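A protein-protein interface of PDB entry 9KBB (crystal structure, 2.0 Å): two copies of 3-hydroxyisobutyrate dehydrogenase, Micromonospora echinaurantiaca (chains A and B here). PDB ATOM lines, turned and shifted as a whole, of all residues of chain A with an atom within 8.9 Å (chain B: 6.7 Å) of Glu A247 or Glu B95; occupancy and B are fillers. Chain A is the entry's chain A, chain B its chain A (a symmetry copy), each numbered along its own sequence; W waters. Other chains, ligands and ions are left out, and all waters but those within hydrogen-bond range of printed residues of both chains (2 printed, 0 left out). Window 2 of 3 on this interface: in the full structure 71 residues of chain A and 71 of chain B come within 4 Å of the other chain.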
ATOM      1  N   MET A 186       6.430  14.448   9.199  1.00  0.00           N
ATOM      2  CA  MET A 186       6.306  13.064   8.748  1.00  0.00           C
ATOM      3  C   MET A 186       5.293  12.297   9.592  1.00  0.00           C
ATOM      4  O   MET A 186       4.452  11.565   9.059  1.00  0.00           O
ATOM      5  CB  MET A 186       7.668  12.367   8.789  1.00  0.00           C
ATOM      6  CG  MET A 186       8.728  13.020   7.924  1.00  0.00           C
ATOM      7  SD  MET A 186      10.276  12.089   7.960  1.00  0.00           S
ATOM      8  CE  MET A 186       9.768  10.532   7.225  1.00  0.00           C
ATOM      9  N   ALA A 189       1.678  13.605   8.989  1.00  0.00           N
ATOM     10  CA  ALA A 189       1.073  13.102   7.759  1.00  0.00           C
ATOM     11  C   ALA A 189       0.553  11.678   7.932  1.00  0.00           C
ATOM     12  O   ALA A 189      -0.350  11.257   7.201  1.00  0.00           O
ATOM     13  CB  ALA A 189       2.082  13.164   6.616  1.00  0.00           C
ATOM     14  N   ALA A 190       1.097  10.928   8.889  1.00  0.00           N
ATOM     15  CA  ALA A 190       0.609   9.589   9.196  1.00  0.00           C
ATOM     16  C   ALA A 190      -0.476   9.588  10.269  1.00  0.00           C
ATOM     17  O   ALA A 190      -0.896   8.510  10.705  1.00  0.00           O
ATOM     18  CB  ALA A 190       1.770   8.693   9.633  1.00  0.00           C
ATOM     19  N   GLY A 239      18.394   7.924   1.660  1.00  0.00           N
ATOM     20  CA  GLY A 239      17.424   7.810   0.581  1.00  0.00           C
ATOM     21  C   GLY A 239      16.069   7.330   1.047  1.00  0.00           C
ATOM     22  O   GLY A 239      15.033   7.741   0.510  1.00  0.00           O
ATOM     23  N   ASN A 240      16.038   6.433   2.038  1.00  0.00           N
ATOM     24  CA  ASN A 240      14.768   5.992   2.603  1.00  0.00           C
ATOM     25  C   ASN A 240      14.041   7.143   3.286  1.00  0.00           C
ATOM     26  O   ASN A 240      12.809   7.230   3.238  1.00  0.00           O
ATOM     27  CB  ASN A 240      15.001   4.855   3.597  1.00  0.00           C
ATOM     28  CG  ASN A 240      15.398   3.561   2.922  1.00  0.00           C
ATOM     29  OD1 ASN A 240      14.966   3.274   1.807  1.00  0.00           O
ATOM     30  ND2 ASN A 240      16.229   2.771   3.595  1.00  0.00           N
ATOM     31  N   LEU A 241      14.794   8.018   3.952  1.00  0.00           N
ATOM     32  CA  LEU A 241      14.193   9.184   4.588  1.00  0.00           C
ATOM     33  C   LEU A 241      13.539  10.091   3.555  1.00  0.00           C
ATOM     34  O   LEU A 241      12.435  10.602   3.775  1.00  0.00           O
ATOM     35  CB  LEU A 241      15.258   9.945   5.375  1.00  0.00           C
ATOM     36  CG  LEU A 241      14.871  11.269   6.042  1.00  0.00           C
ATOM     37  CD1 LEU A 241      13.539  11.185   6.792  1.00  0.00           C
ATOM     38  CD2 LEU A 241      15.989  11.747   6.960  1.00  0.00           C
ATOM     39  N   LEU A 242      14.206  10.297   2.419  1.00  0.00           N
ATOM     40  CA  LEU A 242      13.633  11.123   1.362  1.00  0.00           C
ATOM     41  C   LEU A 242      12.393  10.462   0.772  1.00  0.00           C
ATOM     42  O   LEU A 242      11.368  11.119   0.546  1.00  0.00           O
ATOM     43  CB  LEU A 242      14.680  11.367   0.278  1.00  0.00           C
ATOM     44  CG  LEU A 242      15.916  12.133   0.732  1.00  0.00           C
ATOM     45  CD1 LEU A 242      16.884  12.204  -0.420  1.00  0.00           C
ATOM     46  CD2 LEU A 242      15.545  13.527   1.212  1.00  0.00           C
ATOM     47  N   ALA A 243      12.477   9.158   0.511  1.00  0.00           N
ATOM     48  CA  ALA A 243      11.355   8.443  -0.086  1.00  0.00           C
ATOM     49  C   ALA A 243      10.150   8.430   0.850  1.00  0.00           C
ATOM     50  O   ALA A 243       9.010   8.643   0.418  1.00  0.00           O
ATOM     51  CB  ALA A 243      11.782   7.021  -0.443  1.00  0.00           C
ATOM     52  N   ALA A 244      10.384   8.182   2.140  1.00  0.00           N
ATOM     53  CA  ALA A 244       9.275   8.165   3.088  1.00  0.00           C
ATOM     54  C   ALA A 244       8.638   9.545   3.215  1.00  0.00           C
ATOM     55  O   ALA A 244       7.421   9.661   3.402  1.00  0.00           O
ATOM     56  CB  ALA A 244       9.754   7.664   4.447  1.00  0.00           C
ATOM     57  N   SER A 245       9.444  10.604   3.110  1.00  0.00           N
ATOM     58  CA  SER A 245       8.891  11.955   3.129  1.00  0.00           C
ATOM     59  C   SER A 245       7.959  12.171   1.938  1.00  0.00           C
ATOM     60  O   SER A 245       6.848  12.691   2.088  1.00  0.00           O
ATOM     61  CB  SER A 245      10.025  12.984   3.138  1.00  0.00           C
ATOM     62  OG  SER A 245      10.835  12.855   4.300  1.00  0.00           O
ATOM     63  N   ARG A 246       8.399  11.760   0.745  1.00  0.00           N
ATOM     64  CA  ARG A 246       7.545  11.886  -0.432  1.00  0.00           C
ATOM     65  C   ARG A 246       6.289  11.036  -0.285  1.00  0.00           C
ATOM     66  O   ARG A 246       5.200  11.448  -0.697  1.00  0.00           O
ATOM     67  CB  ARG A 246       8.315  11.508  -1.704  1.00  0.00           C
ATOM     68  CG  ARG A 246       9.638  12.244  -1.846  1.00  0.00           C
ATOM     69  CD  ARG A 246      10.369  11.929  -3.146  1.00  0.00           C
ATOM     70  NE  ARG A 246      11.273  13.025  -3.464  1.00  0.00           N
ATOM     71  CZ  ARG A 246      12.546  13.087  -3.101  1.00  0.00           C
ATOM     72  NH1 ARG A 246      13.189  12.016  -2.656  1.00  0.00           N
ATOM     73  NH2 ARG A 246      13.196  14.244  -3.214  1.00  0.00           N
ATOM     74  N   GLU A 247       6.426   9.857   0.325  1.00  0.00           N
ATOM     75  CA  GLU A 247       5.272   9.004   0.580  1.00  0.00           C
ATOM     76  C   GLU A 247       4.204   9.745   1.371  1.00  0.00           C
ATOM     77  O   GLU A 247       3.008   9.618   1.090  1.00  0.00           O
ATOM     78  CB  GLU A 247       5.712   7.747   1.334  1.00  0.00           C
ATOM     79  CG  GLU A 247       6.255   6.640   0.455  1.00  0.00           C
ATOM     80  CD  GLU A 247       6.723   5.442   1.263  1.00  0.00           C
ATOM     81  OE1 GLU A 247       6.463   5.400   2.488  1.00  0.00           O
ATOM     82  OE2 GLU A 247       7.335   4.529   0.670  1.00  0.00           O
ATOM     83  N   GLY A 248       4.615  10.537   2.355  1.00  0.00           N
ATOM     84  CA  GLY A 248       3.676  11.289   3.152  1.00  0.00           C
ATOM     85  C   GLY A 248       3.325  12.664   2.631  1.00  0.00           C
ATOM     86  O   GLY A 248       2.603  13.396   3.313  1.00  0.00           O
ATOM     87  N   GLY A 249       3.799  13.040   1.444  1.00  0.00           N
ATOM     88  CA  GLY A 249       3.530  14.370   0.930  1.00  0.00           C
ATOM     89  C   GLY A 249       4.272  15.460   1.667  1.00  0.00           C
ATOM     90  O   GLY A 249       3.811  16.605   1.703  1.00  0.00           O
ATOM     91  N   VAL A 250       5.412  15.130   2.266  1.00  0.00           N
ATOM     92  CA  VAL A 250       6.206  16.080   3.035  1.00  0.00           C
ATOM     93  C   VAL A 250       7.372  16.544   2.175  1.00  0.00           C
ATOM     94  O   VAL A 250       8.103  15.719   1.607  1.00  0.00           O
ATOM     95  CB  VAL A 250       6.711  15.459   4.350  1.00  0.00           C
ATOM     96  CG1 VAL A 250       7.600  16.452   5.095  1.00  0.00           C
ATOM     97  CG2 VAL A 250       5.547  15.006   5.221  1.00  0.00           C
ATOM     98  N   SER A 251       7.543  17.861   2.080  1.00  0.00           N
ATOM     99  CA  SER A 251       8.665  18.431   1.346  1.00  0.00           C
ATOM    100  C   SER A 251       9.989  17.916   1.901  1.00  0.00           C
ATOM    101  O   SER A 251      10.127  17.689   3.106  1.00  0.00           O
ATOM    102  CB  SER A 251       8.611  19.957   1.434  1.00  0.00           C
ATOM    103  OG  SER A 251       9.822  20.543   0.996  1.00  0.00           O
ATOM    104  N   THR A 252      10.968  17.728   1.010  1.00  0.00           N
ATOM    105  CA  THR A 252      12.311  17.309   1.396  1.00  0.00           C
ATOM    106  C   THR A 252      13.275  18.480   1.516  1.00  0.00           C
ATOM    107  O   THR A 252      14.479  18.259   1.679  1.00  0.00           O
ATOM    108  CB  THR A 252      12.873  16.306   0.382  1.00  0.00           C
ATOM    109  OG1 THR A 252      12.886  16.904  -0.920  1.00  0.00           O
ATOM    110  CG2 THR A 252      12.028  15.041   0.336  1.00  0.00           C
ATOM    111  N   GLY B  92      13.950   0.498   5.472  1.00  0.00           N
ATOM    112  CA  GLY B  92      12.993   0.701   4.408  1.00  0.00           C
ATOM    113  C   GLY B  92      12.015   1.788   4.777  1.00  0.00           C
ATOM    114  O   GLY B  92      12.184   2.486   5.778  1.00  0.00           O
ATOM    115  N   THR B  93      10.979   1.916   3.957  1.00  0.00           N
ATOM    116  CA  THR B  93       9.976   2.943   4.171  1.00  0.00           C
ATOM    117  C   THR B  93       8.750   2.369   4.872  1.00  0.00           C
ATOM    118  O   THR B  93       8.570   1.149   4.936  1.00  0.00           O
ATOM    119  CB  THR B  93       9.563   3.576   2.836  1.00  0.00           C
ATOM    120  OG1 THR B  93       8.736   2.667   2.110  1.00  0.00           O
ATOM    121  CG2 THR B  93      10.790   3.922   1.998  1.00  0.00           C
ATOM    122  N   PRO B  94       7.886   3.228   5.426  1.00  0.00           N
ATOM    123  CA  PRO B  94       6.653   2.709   6.047  1.00  0.00           C
ATOM    124  C   PRO B  94       5.769   1.933   5.082  1.00  0.00           C
ATOM    125  O   PRO B  94       5.194   0.907   5.465  1.00  0.00           O
ATOM    126  CB  PRO B  94       5.982   3.987   6.565  1.00  0.00           C
ATOM    127  CG  PRO B  94       7.143   4.898   6.862  1.00  0.00           C
ATOM    128  CD  PRO B  94       8.073   4.665   5.704  1.00  0.00           C
ATOM    129  N   GLU B  95       5.638   2.394   3.834  1.00  0.00           N
ATOM    130  CA  GLU B  95       4.763   1.703   2.891  1.00  0.00           C
ATOM    131  C   GLU B  95       5.342   0.352   2.483  1.00  0.00           C
ATOM    132  O   GLU B  95       4.597  -0.620   2.311  1.00  0.00           O
ATOM    133  CB  GLU B  95       4.516   2.577   1.664  1.00  0.00           C
ATOM    134  CG  GLU B  95       3.559   3.726   1.923  1.00  0.00           C
ATOM    135  CD  GLU B  95       2.127   3.255   2.075  1.00  0.00           C
ATOM    136  OE1 GLU B  95       1.575   2.706   1.097  1.00  0.00           O
ATOM    137  OE2 GLU B  95       1.561   3.429   3.175  1.00  0.00           O
ATOM    138  N   GLN B  96       6.663   0.276   2.303  1.00  0.00           N
ATOM    139  CA  GLN B  96       7.288  -1.006   2.000  1.00  0.00           C
ATOM    140  C   GLN B  96       7.039  -2.014   3.115  1.00  0.00           C
ATOM    141  O   GLN B  96       6.823  -3.204   2.849  1.00  0.00           O
ATOM    142  CB  GLN B  96       8.784  -0.817   1.771  1.00  0.00           C
ATOM    143  CG  GLN B  96       9.117  -0.078   0.490  1.00  0.00           C
ATOM    144  CD  GLN B  96      10.585   0.279   0.402  1.00  0.00           C
ATOM    145  OE1 GLN B  96      11.290   0.325   1.413  1.00  0.00           O
ATOM    146  NE2 GLN B  96      11.062   0.512  -0.814  1.00  0.00           N
ATOM    147  N   ALA B  97       7.056  -1.554   4.370  1.00  0.00           N
ATOM    148  CA  ALA B  97       6.785  -2.447   5.492  1.00  0.00           C
ATOM    149  C   ALA B  97       5.333  -2.918   5.485  1.00  0.00           C
ATOM    150  O   ALA B  97       5.044  -4.087   5.772  1.00  0.00           O
ATOM    151  CB  ALA B  97       7.121  -1.745   6.807  1.00  0.00           C
ATOM    152  N   ARG B  98       4.401  -2.014   5.166  1.00  0.00           N
ATOM    153  CA  ARG B  98       2.987  -2.381   5.125  1.00  0.00           C
ATOM    154  C   ARG B  98       2.692  -3.335   3.972  1.00  0.00           C
ATOM    155  O   ARG B  98       1.825  -4.212   4.088  1.00  0.00           O
ATOM    156  CB  ARG B  98       2.127  -1.122   5.013  1.00  0.00           C
ATOM    157  CG  ARG B  98       2.224  -0.203   6.215  1.00  0.00           C
ATOM    158  CD  ARG B  98       1.513   1.112   5.943  1.00  0.00           C
ATOM    159  NE  ARG B  98       1.655   2.046   7.052  1.00  0.00           N
ATOM    160  CZ  ARG B  98       2.094   3.288   6.930  1.00  0.00           C
ATOM    161  NH1 ARG B  98       2.438   3.785   5.753  1.00  0.00           N
ATOM    162  NH2 ARG B  98       2.188   4.054   8.014  1.00  0.00           N
ATOM    163  N   ARG B  99       3.398  -3.175   2.851  1.00  0.00           N
ATOM    164  CA  ARG B  99       3.222  -4.086   1.725  1.00  0.00           C
ATOM    165  C   ARG B  99       3.795  -5.463   2.041  1.00  0.00           C
ATOM    166  O   ARG B  99       3.237  -6.488   1.630  1.00  0.00           O
ATOM    167  CB  ARG B  99       3.884  -3.501   0.476  1.00  0.00           C
ATOM    168  CG  ARG B  99       3.222  -2.237  -0.098  1.00  0.00           C
ATOM    169  CD  ARG B  99       1.736  -2.381  -0.438  1.00  0.00           C
ATOM    170  NE  ARG B  99       0.847  -2.253   0.710  1.00  0.00           N
ATOM    171  CZ  ARG B  99       0.448  -1.106   1.241  1.00  0.00           C
ATOM    172  NH1 ARG B  99       0.948   0.053   0.841  1.00  0.00           N
ATOM    173  NH2 ARG B  99      -0.469  -1.123   2.207  1.00  0.00           N
ATOM    174  N   LEU B 100       4.912  -5.502   2.771  1.00  0.00           N
ATOM    175  CA  LEU B 100       5.505  -6.779   3.154  1.00  0.00           C
ATOM    176  C   LEU B 100       4.615  -7.528   4.140  1.00  0.00           C
ATOM    177  O   LEU B 100       4.517  -8.761   4.082  1.00  0.00           O
ATOM    178  CB  LEU B 100       6.895  -6.554   3.748  1.00  0.00           C
ATOM    179  CG  LEU B 100       7.650  -7.828   4.144  1.00  0.00           C
ATOM    180  CD1 LEU B 100       7.730  -8.834   2.989  1.00  0.00           C
ATOM    181  CD2 LEU B 100       9.037  -7.489   4.678  1.00  0.00           C
ATOM    182  N   GLU B 102       1.348  -7.494   4.223  1.00  0.00           N
ATOM    183  CA  GLU B 102       0.280  -8.116   3.447  1.00  0.00           C
ATOM    184  C   GLU B 102       0.797  -9.321   2.661  1.00  0.00           C
ATOM    185  O   GLU B 102       0.152 -10.374   2.620  1.00  0.00           O
ATOM    186  CB  GLU B 102      -0.356  -7.076   2.524  1.00  0.00           C
ATOM    187  CG  GLU B 102      -0.962  -5.899   3.277  1.00  0.00           C
ATOM    188  CD  GLU B 102      -1.033  -4.633   2.448  1.00  0.00           C
ATOM    189  OE1 GLU B 102      -0.545  -4.639   1.296  1.00  0.00           O
ATOM    190  OE2 GLU B 102      -1.579  -3.630   2.953  1.00  0.00           O
ATOM    191  N   GLY B 160       3.927  -0.179   9.355  1.00  0.00           N
ATOM    192  CA  GLY B 160       4.832   0.879   8.973  1.00  0.00           C
ATOM    193  C   GLY B 160       5.250   1.819  10.084  1.00  0.00           C
ATOM    194  O   GLY B 160       5.929   2.812   9.804  1.00  0.00           O
ATOM    195  N   ALA B 163       9.347   1.992  10.837  1.00  0.00           N
ATOM    196  CA  ALA B 163      10.096   2.720   9.817  1.00  0.00           C
ATOM    197  C   ALA B 163       9.783   4.212   9.862  1.00  0.00           C
ATOM    198  O   ALA B 163      10.676   5.047   9.685  1.00  0.00           O
ATOM    199  CB  ALA B 163       9.792   2.150   8.432  1.00  0.00           C
ATOM    200  N   SER B 285       0.952  17.830  -0.408  1.00  0.00           N
ATOM    201  CA  SER B 285      -0.166  17.038  -0.907  1.00  0.00           C
ATOM    202  C   SER B 285      -1.485  17.480  -0.266  1.00  0.00           C
ATOM    203  O   SER B 285      -2.557  17.045  -0.678  1.00  0.00           O
ATOM    204  CB  SER B 285       0.076  15.555  -0.642  1.00  0.00           C
ATOM    205  OG  SER B 285       1.141  15.059  -1.443  1.00  0.00           O
ATOM    206  OXT SER B 285      -1.503  18.271   0.677  1.00  0.00           O
HETATM  207  O   HOH W   1       0.756  17.242   2.339  1.00  0.00           O
HETATM  208  O   HOH W   2      13.973   1.026   0.613  1.00  0.00           O
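No position is printed for both chains.
The backbone NH of Thr B93 sits at hydrogen-bond distance from the side-chain amide oxygen of Gln B96, at 3.0 Å. The side-chain carboxylate (OE2) of Glu B95 lies within salt-bridge range of the guanidinium group (NH1) of Arg B98 (2.7 Å). The side-chain carboxylate of Glu B95 lies within salt-bridge range of the guanidinium group of Arg B99, at 2.7 Å.
Among the printed residues, pairs that only touch across the chains: Gly A249 with Ser B285, Ala A244 with Pro B94, Glu A247 with Pro B94 and Asn A240 with Gly B92.
Along chain B the printed residues that touch a printed residue of chain A span positions 92 to 285. Hydrophobic or aromatic side chains of chain A within 4 Å of the printed part of chain B: Ala A244. Among the printed residues, 6 pairs touch across the chains. Among the printed residues, no Asp or Glu carboxylate lies within 4 Å of a Lys or Arg side-chain nitrogen of the other chain.
OE2 of Glu A247 lies within hydrogen-bond range of OG1 of Thr B93 (2.7 Å). The backbone NH (N) of Glu B95 lies within hydrogen-bond range of the side-chain carboxylate (OE1) of Glu A247 (3.4 Å).
Water W2 lies within hydrogen-bond range of OD1 of Asn A240 (2.7 Å) and OE1 of Gln B96 (2.9 Å). Water W1 lies within hydrogen-bond range of the backbone NH (N) of Ser B285 (2.8 Å) and the backbone carbonyl oxygen (O) of Gly A249 (3.2 Å).
Ala A190 touches none of the printed residues of chain B. Printed residues of chain B within 4 Å of Asn A240: Gly B92 (3.7 Å). Printed residues of chain B within 4 Å of Ala A244: Pro B94 (3.7 Å). Of chain B, only Thr B93, Pro B94 and Glu B95 come within 4 Å of Glu A247. Printed residues of chain B within 4 Å of Gly A249: Ser B285 (3.4 Å). Of the printed residues of chain A, Gly B92 touches Asn A240 (3.7 Å). Of the printed residues of chain A, Thr B93 touches Glu A247 (2.7 Å). Pro B94 touches just these residues of chain A: Ala A244 and Glu A247. Printed residues of chain A within 4 Å of Glu B95: Glu A247 (3.4 Å). Arg B98 touches none of the printed residues of chain A. The nearest residue of chain A that does not touch Glu B95 is Ala A244 (6.7 Å).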
